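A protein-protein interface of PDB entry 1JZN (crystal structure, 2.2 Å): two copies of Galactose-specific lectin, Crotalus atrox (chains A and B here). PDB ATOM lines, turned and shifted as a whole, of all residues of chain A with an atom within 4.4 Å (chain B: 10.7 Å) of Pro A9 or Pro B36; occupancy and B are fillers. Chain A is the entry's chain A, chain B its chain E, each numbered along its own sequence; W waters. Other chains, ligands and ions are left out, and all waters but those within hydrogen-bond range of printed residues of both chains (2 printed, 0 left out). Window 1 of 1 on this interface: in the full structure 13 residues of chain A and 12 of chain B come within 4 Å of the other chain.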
ATOM      1  N   CYS A   3     -20.409  11.203  23.555  1.00  0.00           N
ATOM      2  CA  CYS A   3     -18.980  10.905  23.442  1.00  0.00           C
ATOM      3  C   CYS A   3     -18.246  12.054  22.748  1.00  0.00           C
ATOM      4  O   CYS A   3     -18.889  12.950  22.182  1.00  0.00           O
ATOM      5  CB  CYS A   3     -18.799   9.637  22.590  1.00  0.00           C
ATOM      6  SG  CYS A   3     -19.710   8.145  23.150  1.00  0.00           S
ATOM      7  N   LEU A   5     -16.062  13.804  19.789  1.00  0.00           N
ATOM      8  CA  LEU A   5     -16.202  13.668  18.343  1.00  0.00           C
ATOM      9  C   LEU A   5     -15.346  12.534  17.754  1.00  0.00           C
ATOM     10  O   LEU A   5     -15.728  11.896  16.775  1.00  0.00           O
ATOM     11  CB  LEU A   5     -15.814  15.015  17.681  1.00  0.00           C
ATOM     12  CG  LEU A   5     -16.023  15.160  16.164  1.00  0.00           C
ATOM     13  CD1 LEU A   5     -17.550  15.235  15.890  1.00  0.00           C
ATOM     14  CD2 LEU A   5     -15.301  16.424  15.631  1.00  0.00           C
ATOM     15  N   ASP A   6     -14.198  12.282  18.381  1.00  0.00           N
ATOM     16  CA  ASP A   6     -13.241  11.269  17.920  1.00  0.00           C
ATOM     17  C   ASP A   6     -13.605   9.823  18.314  1.00  0.00           C
ATOM     18  O   ASP A   6     -12.898   8.868  17.965  1.00  0.00           O
ATOM     19  CB  ASP A   6     -11.854  11.662  18.468  1.00  0.00           C
ATOM     20  CG  ASP A   6     -10.722  10.832  17.892  1.00  0.00           C
ATOM     21  OD1 ASP A   6     -10.606  10.730  16.655  1.00  0.00           O
ATOM     22  OD2 ASP A   6      -9.928  10.281  18.692  1.00  0.00           O
ATOM     23  N   TRP A   7     -14.721   9.671  19.023  1.00  0.00           N
ATOM     24  CA  TRP A   7     -15.167   8.358  19.486  1.00  0.00           C
ATOM     25  C   TRP A   7     -16.503   7.915  18.902  1.00  0.00           C
ATOM     26  O   TRP A   7     -17.325   8.727  18.521  1.00  0.00           O
ATOM     27  CB  TRP A   7     -15.269   8.350  21.017  1.00  0.00           C
ATOM     28  CG  TRP A   7     -13.945   8.451  21.715  1.00  0.00           C
ATOM     29  CD1 TRP A   7     -13.054   9.493  21.651  1.00  0.00           C
ATOM     30  CD2 TRP A   7     -13.342   7.456  22.560  1.00  0.00           C
ATOM     31  NE1 TRP A   7     -11.933   9.200  22.401  1.00  0.00           N
ATOM     32  CE2 TRP A   7     -12.082   7.960  22.967  1.00  0.00           C
ATOM     33  CE3 TRP A   7     -13.742   6.191  23.007  1.00  0.00           C
ATOM     34  CZ2 TRP A   7     -11.218   7.239  23.804  1.00  0.00           C
ATOM     35  CZ3 TRP A   7     -12.880   5.469  23.841  1.00  0.00           C
ATOM     36  CH2 TRP A   7     -11.632   5.997  24.230  1.00  0.00           C
ATOM     37  N   LEU A   8     -16.711   6.607  18.864  1.00  0.00           N
ATOM     38  CA  LEU A   8     -17.943   6.024  18.346  1.00  0.00           C
ATOM     39  C   LEU A   8     -18.922   5.703  19.488  1.00  0.00           C
ATOM     40  O   LEU A   8     -18.618   4.879  20.334  1.00  0.00           O
ATOM     41  CB  LEU A   8     -17.624   4.716  17.589  1.00  0.00           C
ATOM     42  CG  LEU A   8     -18.790   3.757  17.289  1.00  0.00           C
ATOM     43  CD1 LEU A   8     -19.609   4.296  16.100  1.00  0.00           C
ATOM     44  CD2 LEU A   8     -18.266   2.360  16.969  1.00  0.00           C
ATOM     45  N   PRO A   9     -20.090   6.377  19.536  1.00  0.00           N
ATOM     46  CA  PRO A   9     -21.078   6.104  20.590  1.00  0.00           C
ATOM     47  C   PRO A   9     -21.881   4.850  20.194  1.00  0.00           C
ATOM     48  O   PRO A   9     -22.339   4.740  19.061  1.00  0.00           O
ATOM     49  CB  PRO A   9     -21.973   7.352  20.588  1.00  0.00           C
ATOM     50  CG  PRO A   9     -21.211   8.377  19.718  1.00  0.00           C
ATOM     51  CD  PRO A   9     -20.508   7.528  18.713  1.00  0.00           C
ATOM     52  N   MET A  10     -22.029   3.904  21.117  1.00  0.00           N
ATOM     53  CA  MET A  10     -22.798   2.699  20.843  1.00  0.00           C
ATOM     54  C   MET A  10     -23.388   2.177  22.154  1.00  0.00           C
ATOM     55  O   MET A  10     -22.666   1.961  23.130  1.00  0.00           O
ATOM     56  CB  MET A  10     -21.924   1.612  20.175  1.00  0.00           C
ATOM     57  CG  MET A  10     -22.656   0.342  19.704  1.00  0.00           C
ATOM     58  SD  MET A  10     -21.549  -0.797  18.785  1.00  0.00           S
ATOM     59  CE  MET A  10     -20.558  -1.479  20.117  1.00  0.00           C
ATOM     60  N   LEU A  13     -22.018   3.450  25.573  1.00  0.00           N
ATOM     61  CA  LEU A  13     -20.590   3.584  25.818  1.00  0.00           C
ATOM     62  C   LEU A  13     -19.885   4.214  24.605  1.00  0.00           C
ATOM     63  O   LEU A  13     -20.505   4.462  23.564  1.00  0.00           O
ATOM     64  CB  LEU A  13     -19.981   2.224  26.166  1.00  0.00           C
ATOM     65  CG  LEU A  13     -20.550   1.494  27.390  1.00  0.00           C
ATOM     66  CD1 LEU A  13     -19.957   0.098  27.491  1.00  0.00           C
ATOM     67  CD2 LEU A  13     -20.217   2.267  28.649  1.00  0.00           C
ATOM     68  N   GLU A  51     -21.330  -3.307  13.629  1.00  0.00           N
ATOM     69  CA  GLU A  51     -21.043  -1.871  13.692  1.00  0.00           C
ATOM     70  C   GLU A  51     -19.538  -1.634  13.984  1.00  0.00           C
ATOM     71  O   GLU A  51     -18.892  -0.799  13.346  1.00  0.00           O
ATOM     72  CB  GLU A  51     -21.905  -1.191  14.780  1.00  0.00           C
ATOM     73  CG  GLU A  51     -22.004   0.331  14.639  1.00  0.00           C
ATOM     74  CD  GLU A  51     -22.802   1.010  15.756  1.00  0.00           C
ATOM     75  OE1 GLU A  51     -23.789   0.422  16.264  1.00  0.00           O
ATOM     76  OE2 GLU A  51     -22.452   2.155  16.120  1.00  0.00           O
ATOM     77  N   TYR A  55     -16.684   0.141  11.587  1.00  0.00           N
ATOM     78  CA  TYR A  55     -15.984   1.288  12.145  1.00  0.00           C
ATOM     79  C   TYR A  55     -14.461   1.096  12.032  1.00  0.00           C
ATOM     80  O   TYR A  55     -13.748   1.998  11.582  1.00  0.00           O
ATOM     81  CB  TYR A  55     -16.380   1.487  13.613  1.00  0.00           C
ATOM     82  CG  TYR A  55     -15.392   2.324  14.413  1.00  0.00           C
ATOM     83  CD1 TYR A  55     -14.805   1.817  15.581  1.00  0.00           C
ATOM     84  CD2 TYR A  55     -15.019   3.605  13.989  1.00  0.00           C
ATOM     85  CE1 TYR A  55     -13.868   2.563  16.295  1.00  0.00           C
ATOM     86  CE2 TYR A  55     -14.082   4.355  14.694  1.00  0.00           C
ATOM     87  CZ  TYR A  55     -13.509   3.827  15.837  1.00  0.00           C
ATOM     88  OH  TYR A  55     -12.527   4.525  16.497  1.00  0.00           O
ATOM     89  N   TYR A  59     -11.742   3.373  10.012  1.00  0.00           N
ATOM     90  CA  TYR A  59     -10.750   4.177  10.710  1.00  0.00           C
ATOM     91  C   TYR A  59      -9.416   3.504  11.064  1.00  0.00           C
ATOM     92  O   TYR A  59      -8.581   4.110  11.723  1.00  0.00           O
ATOM     93  CB  TYR A  59     -11.389   4.789  11.964  1.00  0.00           C
ATOM     94  CG  TYR A  59     -12.457   5.824  11.672  1.00  0.00           C
ATOM     95  CD1 TYR A  59     -13.725   5.449  11.211  1.00  0.00           C
ATOM     96  CD2 TYR A  59     -12.194   7.189  11.840  1.00  0.00           C
ATOM     97  CE1 TYR A  59     -14.694   6.403  10.924  1.00  0.00           C
ATOM     98  CE2 TYR A  59     -13.151   8.148  11.554  1.00  0.00           C
ATOM     99  CZ  TYR A  59     -14.401   7.759  11.091  1.00  0.00           C
ATOM    100  OH  TYR A  59     -15.335   8.731  10.762  1.00  0.00           O
ATOM    101  N   ASN B   2     -27.998  18.388  21.807  1.00  0.00           N
ATOM    102  CA  ASN B   2     -27.792  17.038  21.280  1.00  0.00           C
ATOM    103  C   ASN B   2     -27.016  16.995  19.971  1.00  0.00           C
ATOM    104  O   ASN B   2     -26.407  15.971  19.653  1.00  0.00           O
ATOM    105  CB  ASN B   2     -29.131  16.318  21.049  1.00  0.00           C
ATOM    106  CG  ASN B   2     -29.810  15.913  22.339  1.00  0.00           C
ATOM    107  OD1 ASN B   2     -29.147  15.555  23.315  1.00  0.00           O
ATOM    108  ND2 ASN B   2     -31.142  15.952  22.347  1.00  0.00           N
ATOM    109  N   TRP B   7     -27.171  20.934  12.419  1.00  0.00           N
ATOM    110  CA  TRP B   7     -27.727  19.581  12.242  1.00  0.00           C
ATOM    111  C   TRP B   7     -29.123  19.533  12.880  1.00  0.00           C
ATOM    112  O   TRP B   7     -29.412  20.261  13.814  1.00  0.00           O
ATOM    113  CB  TRP B   7     -26.835  18.500  12.895  1.00  0.00           C
ATOM    114  CG  TRP B   7     -25.521  18.245  12.191  1.00  0.00           C
ATOM    115  CD1 TRP B   7     -24.479  19.135  12.019  1.00  0.00           C
ATOM    116  CD2 TRP B   7     -25.109  17.025  11.554  1.00  0.00           C
ATOM    117  NE1 TRP B   7     -23.452  18.537  11.326  1.00  0.00           N
ATOM    118  CE2 TRP B   7     -23.807  17.249  11.022  1.00  0.00           C
ATOM    119  CE3 TRP B   7     -25.713  15.761  11.378  1.00  0.00           C
ATOM    120  CZ2 TRP B   7     -23.095  16.256  10.323  1.00  0.00           C
ATOM    121  CZ3 TRP B   7     -25.004  14.772  10.685  1.00  0.00           C
ATOM    122  CH2 TRP B   7     -23.704  15.029  10.164  1.00  0.00           C
ATOM    123  N   GLY B  12     -33.226  11.281  19.144  1.00  0.00           N
ATOM    124  CA  GLY B  12     -31.924  10.772  19.549  1.00  0.00           C
ATOM    125  C   GLY B  12     -30.781  10.840  18.540  1.00  0.00           C
ATOM    126  O   GLY B  12     -29.632  10.567  18.885  1.00  0.00           O
ATOM    127  N   LEU B  13     -31.063  11.194  17.294  1.00  0.00           N
ATOM    128  CA  LEU B  13     -29.996  11.271  16.293  1.00  0.00           C
ATOM    129  C   LEU B  13     -29.868  12.670  15.714  1.00  0.00           C
ATOM    130  O   LEU B  13     -30.683  13.529  16.004  1.00  0.00           O
ATOM    131  CB  LEU B  13     -30.261  10.266  15.165  1.00  0.00           C
ATOM    132  CG  LEU B  13     -30.020   8.809  15.522  1.00  0.00           C
ATOM    133  CD1 LEU B  13     -30.506   7.918  14.407  1.00  0.00           C
ATOM    134  CD2 LEU B  13     -28.542   8.603  15.770  1.00  0.00           C
ATOM    135  N   CYS B  14     -28.854  12.875  14.879  1.00  0.00           N
ATOM    136  CA  CYS B  14     -28.600  14.174  14.238  1.00  0.00           C
ATOM    137  C   CYS B  14     -28.514  14.015  12.728  1.00  0.00           C
ATOM    138  O   CYS B  14     -27.761  13.189  12.222  1.00  0.00           O
ATOM    139  CB  CYS B  14     -27.297  14.784  14.744  1.00  0.00           C
ATOM    140  SG  CYS B  14     -27.254  14.934  16.559  1.00  0.00           S
ATOM    141  N   GLU B  28     -22.383   7.545   0.988  1.00  0.00           N
ATOM    142  CA  GLU B  28     -22.341   6.703   2.205  1.00  0.00           C
ATOM    143  C   GLU B  28     -20.955   6.856   2.829  1.00  0.00           C
ATOM    144  O   GLU B  28     -20.821   7.112   4.027  1.00  0.00           O
ATOM    145  CB  GLU B  28     -22.492   5.204   1.878  1.00  0.00           C
ATOM    146  CG  GLU B  28     -23.525   4.358   2.655  1.00  0.00           C
ATOM    147  CD  GLU B  28     -23.622   4.587   4.158  1.00  0.00           C
ATOM    148  OE1 GLU B  28     -22.924   3.919   4.959  1.00  0.00           O
ATOM    149  OE2 GLU B  28     -24.441   5.430   4.543  1.00  0.00           O
ATOM    150  N   MET B  29     -19.920   6.647   2.019  1.00  0.00           N
ATOM    151  CA  MET B  29     -18.546   6.753   2.534  1.00  0.00           C
ATOM    152  C   MET B  29     -18.220   8.144   3.086  1.00  0.00           C
ATOM    153  O   MET B  29     -17.506   8.273   4.079  1.00  0.00           O
ATOM    154  CB  MET B  29     -17.524   6.305   1.467  1.00  0.00           C
ATOM    155  CG  MET B  29     -17.170   4.765   1.523  1.00  0.00           C
ATOM    156  SD  MET B  29     -15.799   4.172   2.707  1.00  0.00           S
ATOM    157  CE  MET B  29     -14.250   4.662   1.728  1.00  0.00           C
ATOM    158  N   PHE B  30     -18.768   9.187   2.480  1.00  0.00           N
ATOM    159  CA  PHE B  30     -18.528  10.544   2.975  1.00  0.00           C
ATOM    160  C   PHE B  30     -19.081  10.664   4.411  1.00  0.00           C
ATOM    161  O   PHE B  30     -18.392  11.164   5.328  1.00  0.00           O
ATOM    162  CB  PHE B  30     -19.206  11.571   2.059  1.00  0.00           C
ATOM    163  CG  PHE B  30     -19.094  12.987   2.552  1.00  0.00           C
ATOM    164  CD1 PHE B  30     -19.886  13.439   3.613  1.00  0.00           C
ATOM    165  CD2 PHE B  30     -18.183  13.872   1.970  1.00  0.00           C
ATOM    166  CE1 PHE B  30     -19.774  14.742   4.086  1.00  0.00           C
ATOM    167  CE2 PHE B  30     -18.062  15.190   2.432  1.00  0.00           C
ATOM    168  CZ  PHE B  30     -18.851  15.628   3.485  1.00  0.00           C
ATOM    169  N   CYS B  31     -20.327  10.231   4.591  1.00  0.00           N
ATOM    170  CA  CYS B  31     -20.966  10.251   5.914  1.00  0.00           C
ATOM    171  C   CYS B  31     -20.139   9.400   6.902  1.00  0.00           C
ATOM    172  O   CYS B  31     -19.758   9.882   7.971  1.00  0.00           O
ATOM    173  CB  CYS B  31     -22.413   9.695   5.877  1.00  0.00           C
ATOM    174  SG  CYS B  31     -23.682  10.586   4.878  1.00  0.00           S
ATOM    175  N   ARG B  32     -19.848   8.152   6.537  1.00  0.00           N
ATOM    176  CA  ARG B  32     -19.089   7.248   7.408  1.00  0.00           C
ATOM    177  C   ARG B  32     -17.749   7.823   7.853  1.00  0.00           C
ATOM    178  O   ARG B  32     -17.370   7.694   9.028  1.00  0.00           O
ATOM    179  CB  ARG B  32     -18.858   5.905   6.714  1.00  0.00           C
ATOM    180  CG  ARG B  32     -20.155   5.145   6.429  1.00  0.00           C
ATOM    181  CD  ARG B  32     -20.104   3.770   7.035  1.00  0.00           C
ATOM    182  NE  ARG B  32     -18.983   3.003   6.511  1.00  0.00           N
ATOM    183  CZ  ARG B  32     -19.040   2.240   5.431  1.00  0.00           C
ATOM    184  NH1 ARG B  32     -20.175   2.133   4.763  1.00  0.00           N
ATOM    185  NH2 ARG B  32     -17.958   1.602   5.007  1.00  0.00           N
ATOM    186  N   LYS B  33     -17.052   8.473   6.922  1.00  0.00           N
ATOM    187  CA  LYS B  33     -15.756   9.068   7.211  1.00  0.00           C
ATOM    188  C   LYS B  33     -15.850  10.437   7.866  1.00  0.00           C
ATOM    189  O   LYS B  33     -14.821  11.020   8.210  1.00  0.00           O
ATOM    190  CB  LYS B  33     -14.903   9.202   5.931  1.00  0.00           C
ATOM    191  CG  LYS B  33     -14.619   7.891   5.176  1.00  0.00           C
ATOM    192  CD  LYS B  33     -13.969   6.786   6.040  1.00  0.00           C
ATOM    193  CE  LYS B  33     -12.511   7.079   6.473  1.00  0.00           C
ATOM    194  NZ  LYS B  33     -12.397   7.861   7.749  1.00  0.00           N
ATOM    195  N   TYR B  34     -17.052  10.972   8.034  1.00  0.00           N
ATOM    196  CA  TYR B  34     -17.160  12.293   8.664  1.00  0.00           C
ATOM    197  C   TYR B  34     -16.759  12.206  10.145  1.00  0.00           C
ATOM    198  O   TYR B  34     -15.850  12.907  10.594  1.00  0.00           O
ATOM    199  CB  TYR B  34     -18.577  12.871   8.523  1.00  0.00           C
ATOM    200  CG  TYR B  34     -18.686  14.268   9.068  1.00  0.00           C
ATOM    201  CD1 TYR B  34     -19.366  14.537  10.258  1.00  0.00           C
ATOM    202  CD2 TYR B  34     -18.046  15.335   8.413  1.00  0.00           C
ATOM    203  CE1 TYR B  34     -19.397  15.851  10.780  1.00  0.00           C
ATOM    204  CE2 TYR B  34     -18.070  16.616   8.914  1.00  0.00           C
ATOM    205  CZ  TYR B  34     -18.738  16.882  10.083  1.00  0.00           C
ATOM    206  OH  TYR B  34     -18.764  18.192  10.518  1.00  0.00           O
ATOM    207  N   LYS B  35     -17.444  11.369  10.905  1.00  0.00           N
ATOM    208  CA  LYS B  35     -17.092  11.148  12.318  1.00  0.00           C
ATOM    209  C   LYS B  35     -17.553   9.691  12.577  1.00  0.00           C
ATOM    210  O   LYS B  35     -18.407   9.176  11.854  1.00  0.00           O
ATOM    211  CB  LYS B  35     -17.818  12.124  13.265  1.00  0.00           C
ATOM    212  CG  LYS B  35     -19.203  11.625  13.691  1.00  0.00           C
ATOM    213  CD  LYS B  35     -19.764  12.338  14.900  1.00  0.00           C
ATOM    214  CE  LYS B  35     -19.130  11.867  16.201  1.00  0.00           C
ATOM    215  NZ  LYS B  35     -19.543  10.507  16.651  1.00  0.00           N
ATOM    216  N   PRO B  36     -16.976   9.006  13.578  1.00  0.00           N
ATOM    217  CA  PRO B  36     -17.399   7.619  13.830  1.00  0.00           C
ATOM    218  C   PRO B  36     -18.893   7.504  14.185  1.00  0.00           C
ATOM    219  O   PRO B  36     -19.368   8.198  15.077  1.00  0.00           O
ATOM    220  CB  PRO B  36     -16.495   7.181  14.996  1.00  0.00           C
ATOM    221  CG  PRO B  36     -15.234   8.043  14.806  1.00  0.00           C
ATOM    222  CD  PRO B  36     -15.819   9.381  14.417  1.00  0.00           C
ATOM    223  N   GLY B  37     -19.621   6.644  13.478  1.00  0.00           N
ATOM    224  CA  GLY B  37     -21.036   6.443  13.776  1.00  0.00           C
ATOM    225  C   GLY B  37     -22.055   7.148  12.897  1.00  0.00           C
ATOM    226  O   GLY B  37     -23.191   7.357  13.316  1.00  0.00           O
ATOM    227  N   CYS B  38     -21.660   7.521  11.689  1.00  0.00           N
ATOM    228  CA  CYS B  38     -22.555   8.216  10.763  1.00  0.00           C
ATOM    229  C   CYS B  38     -22.844   7.329   9.562  1.00  0.00           C
ATOM    230  O   CYS B  38     -22.076   6.446   9.250  1.00  0.00           O
ATOM    231  CB  CYS B  38     -21.907   9.503  10.239  1.00  0.00           C
ATOM    232  SG  CYS B  38     -21.346  10.745  11.450  1.00  0.00           S
ATOM    233  N   HIS B  39     -23.952   7.594   8.881  1.00  0.00           N
ATOM    234  CA  HIS B  39     -24.349   6.838   7.701  1.00  0.00           C
ATOM    235  C   HIS B  39     -25.314   7.711   6.938  1.00  0.00           C
ATOM    236  O   HIS B  39     -25.720   8.765   7.422  1.00  0.00           O
ATOM    237  CB  HIS B  39     -25.138   5.567   8.098  1.00  0.00           C
ATOM    238  CG  HIS B  39     -24.292   4.458   8.654  1.00  0.00           C
ATOM    239  ND1 HIS B  39     -24.193   4.198  10.004  1.00  0.00           N
ATOM    240  CD2 HIS B  39     -23.500   3.551   8.040  1.00  0.00           C
ATOM    241  CE1 HIS B  39     -23.382   3.175  10.197  1.00  0.00           C
ATOM    242  NE2 HIS B  39     -22.947   2.764   9.023  1.00  0.00           N
ATOM    243  N   ASP B  83     -27.203   1.733   8.023  1.00  0.00           N
ATOM    244  CA  ASP B  83     -26.942   1.779   9.473  1.00  0.00           C
ATOM    245  C   ASP B  83     -27.434   0.477  10.164  1.00  0.00           C
ATOM    246  O   ASP B  83     -27.453   0.378  11.400  1.00  0.00           O
ATOM    247  CB  ASP B  83     -27.613   3.013  10.122  1.00  0.00           C
ATOM    248  CG  ASP B  83     -29.137   2.899  10.174  1.00  0.00           C
ATOM    249  OD1 ASP B  83     -29.779   3.769  10.780  1.00  0.00           O
ATOM    250  OD2 ASP B  83     -29.696   1.951   9.585  1.00  0.00           O
ATOM    251  N   ARG B  84     -27.839  -0.511   9.358  1.00  0.00           N
ATOM    252  CA  ARG B  84     -28.313  -1.809   9.871  1.00  0.00           C
ATOM    253  C   ARG B  84     -29.565  -1.767  10.757  1.00  0.00           C
ATOM    254  O   ARG B  84     -29.919  -2.772  11.375  1.00  0.00           O
ATOM    255  CB  ARG B  84     -27.171  -2.548  10.608  1.00  0.00           C
ATOM    256  CG  ARG B  84     -26.025  -3.024   9.680  1.00  0.00           C
ATOM    257  CD  ARG B  84     -24.754  -3.475  10.446  1.00  0.00           C
ATOM    258  NE  ARG B  84     -24.026  -2.337  11.002  1.00  0.00           N
ATOM    259  CZ  ARG B  84     -23.160  -1.595  10.322  1.00  0.00           C
ATOM    260  NH1 ARG B  84     -22.875  -1.875   9.055  1.00  0.00           N
ATOM    261  NH2 ARG B  84     -22.628  -0.524  10.893  1.00  0.00           N
ATOM    262  N   GLN B 132     -26.695  11.021   8.749  1.00  0.00           N
ATOM    263  CA  GLN B 132     -27.255  10.752  10.065  1.00  0.00           C
ATOM    264  C   GLN B 132     -26.076  10.363  10.977  1.00  0.00           C
ATOM    265  O   GLN B 132     -25.271   9.499  10.633  1.00  0.00           O
ATOM    266  CB  GLN B 132     -28.233   9.586   9.937  1.00  0.00           C
ATOM    267  CG  GLN B 132     -28.578   8.862  11.208  1.00  0.00           C
ATOM    268  CD  GLN B 132     -29.246   7.533  10.898  1.00  0.00           C
ATOM    269  OE1 GLN B 132     -30.338   7.510  10.334  1.00  0.00           O
ATOM    270  NE2 GLN B 132     -28.578   6.420  11.237  1.00  0.00           N
ATOM    271  N   CYS B 133     -25.961  10.998  12.126  1.00  0.00           N
ATOM    272  CA  CYS B 133     -24.866  10.680  13.027  1.00  0.00           C
ATOM    273  C   CYS B 133     -25.342  10.618  14.454  1.00  0.00           C
ATOM    274  O   CYS B 133     -26.340  11.214  14.822  1.00  0.00           O
ATOM    275  CB  CYS B 133     -23.777  11.750  13.016  1.00  0.00           C
ATOM    276  SG  CYS B 133     -22.841  12.099  11.500  1.00  0.00           S
ATOM    277  N   LYS B 134     -24.581   9.896  15.256  1.00  0.00           N
ATOM    278  CA  LYS B 134     -24.837   9.810  16.674  1.00  0.00           C
ATOM    279  C   LYS B 134     -23.680  10.657  17.231  1.00  0.00           C
ATOM    280  O   LYS B 134     -22.521  10.380  16.930  1.00  0.00           O
ATOM    281  CB  LYS B 134     -24.710   8.361  17.152  1.00  0.00           C
ATOM    282  CG  LYS B 134     -25.741   7.392  16.556  1.00  0.00           C
ATOM    283  CD  LYS B 134     -25.141   6.020  16.219  1.00  0.00           C
ATOM    284  CE  LYS B 134     -24.795   5.187  17.454  1.00  0.00           C
ATOM    285  NZ  LYS B 134     -23.988   3.963  17.105  1.00  0.00           N
ATOM    286  N   PHE B 135     -23.989  11.713  17.977  1.00  0.00           N
ATOM    287  CA  PHE B 135     -22.938  12.529  18.596  1.00  0.00           C
ATOM    288  C   PHE B 135     -22.886  12.200  20.103  1.00  0.00           C
ATOM    289  O   PHE B 135     -21.774  12.082  20.655  1.00  0.00           O
ATOM    290  CB  PHE B 135     -23.184  14.031  18.377  1.00  0.00           C
ATOM    291  CG  PHE B 135     -22.860  14.511  16.971  1.00  0.00           C
ATOM    292  CD1 PHE B 135     -23.792  14.381  15.939  1.00  0.00           C
ATOM    293  CD2 PHE B 135     -21.622  15.096  16.690  1.00  0.00           C
ATOM    294  CE1 PHE B 135     -23.500  14.834  14.638  1.00  0.00           C
ATOM    295  CE2 PHE B 135     -21.313  15.549  15.400  1.00  0.00           C
ATOM    296  CZ  PHE B 135     -22.261  15.417  14.364  1.00  0.00           C
ATOM    297  OXT PHE B 135     -23.969  12.047  20.715  1.00  0.00           O
HETATM  298  O   HOH W   1     -19.212  11.221  19.093  1.00  0.00           O
HETATM  299  O   HOH W   2     -19.524  14.092  19.633  1.00  0.00           O
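The chain-end carboxylate (O) of Phe B135 sits at hydrogen-bond distance from the backbone NH (N) of Cys A3, 3.3 Å away.
O of Trp A7 sits at hydrogen-bond distance from NZ of Lys B35 (3.4 Å).
O of Pro A9 sits at hydrogen-bond distance from NZ of Lys B134 (2.7 Å).
OE2 of Glu A51 is in salt-bridge range of NZ of Lys B134.
O of Arg B32 is in hydrogen-bond range of OH of Tyr A59 (2.9 Å).
OH of Tyr A59 sits close to O of Lys B33 (3.5 Å).
OH of Tyr A59 lies close to O of Lys B35.
N of Pro B36 sits close to OH of Tyr A59.
The guanidinium group (NH1) of Arg B32 is in salt-bridge range of the side-chain carboxylate (OE1) of Glu B28 (3.3 Å).
The side-chain amino group of Lys B35 is in hydrogen-bond range of the backbone carbonyl oxygen of Lys B134.
O of Gly B37 is in hydrogen-bond range of N of Lys B134, at 3.5 Å.
The side-chain sulfur (SG) of Cys B133 is disulfide-bonded to the side-chain sulfur (SG) of Cys B38, 2.0 Å away.
Among the printed residues, pairs that only touch across the chains: Leu A5 with Lys B35 (3.5 Å), Leu A5 with Pro B36 (3.4 Å), Leu A5 with Phe B135 (3.8 Å), Trp A7 with Pro B36 (3.9 Å), Leu A8 with Pro B36 (3.8 Å), Leu A8 with Gly B37 (3.5 Å), Pro A9 with Lys B35 (3.7 Å), Pro A9 with Pro B36 (3.9 Å), Pro A9 with Phe B135 (3.9 Å), Glu A51 with Arg B84 (3.5 Å), Tyr A55 with Pro B36 (3.7 Å) and Tyr A59 with Tyr B34 (3.8 Å).
Of chain B, only Phe B135 comes within 4 Å of Cys A3.
Printed residues of chain B within 4 Å of Leu A5: Lys B35 (3.5 Å), Pro B36 (3.4 Å) and Phe B135 (3.8 Å).
Of chain B, only Lys B35 (3.7 Å), Pro B36 (3.9 Å), Lys B134 (2.7 Å) and Phe B135 (3.9 Å) come within 4 Å of Pro A9.
Met A10 touches none of the printed residues of chain B.
Printed residues of chain B within 4 Å of Glu A51: Arg B84 and Lys B134.
Of the printed residues of chain B, Tyr A55 touches Pro B36 (3.7 Å).
Printed residues of chain A within 4 Å of Arg B32: Tyr A59 (2.9 Å).
Of the printed residues of chain A, Pro B36 touches Leu A5 (3.4 Å), Trp A7 (3.9 Å), Leu A8 (3.8 Å), Pro A9 (3.9 Å), Tyr A55 (3.7 Å) and Tyr A59 (3.3 Å).
Of the printed residues of chain A, Gly B37 touches Leu A8.
Asp B83 touches none of the printed residues of chain A.
The nearest residue of chain B that does not touch Pro A9 is Gly B37 (5.1 Å).
The nearest printed residue of chain A that does not touch Pro B36 is Asp A6 (4.01 Å).
Hydrophobic or aromatic side chains of chain A that line the printed part of chain B: Leu A5, Leu A8, Pro A9, Tyr A55 and Tyr A59.
Among the printed residues, 20 pairs touch across the chains.
Positions printed for both chains: 7 and 13.
Water W1 lies within hydrogen-bond range of NZ of Lys B35, O of Phe B135 and O of Trp A7.
Water W2 lies within hydrogen-bond range of the backbone carbonyl oxygen of Cys A3 (2.9 Å), the chain-end carboxylate of Phe B135 (3.2 Å) and the backbone NH of Leu A5 (3.5 Å).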
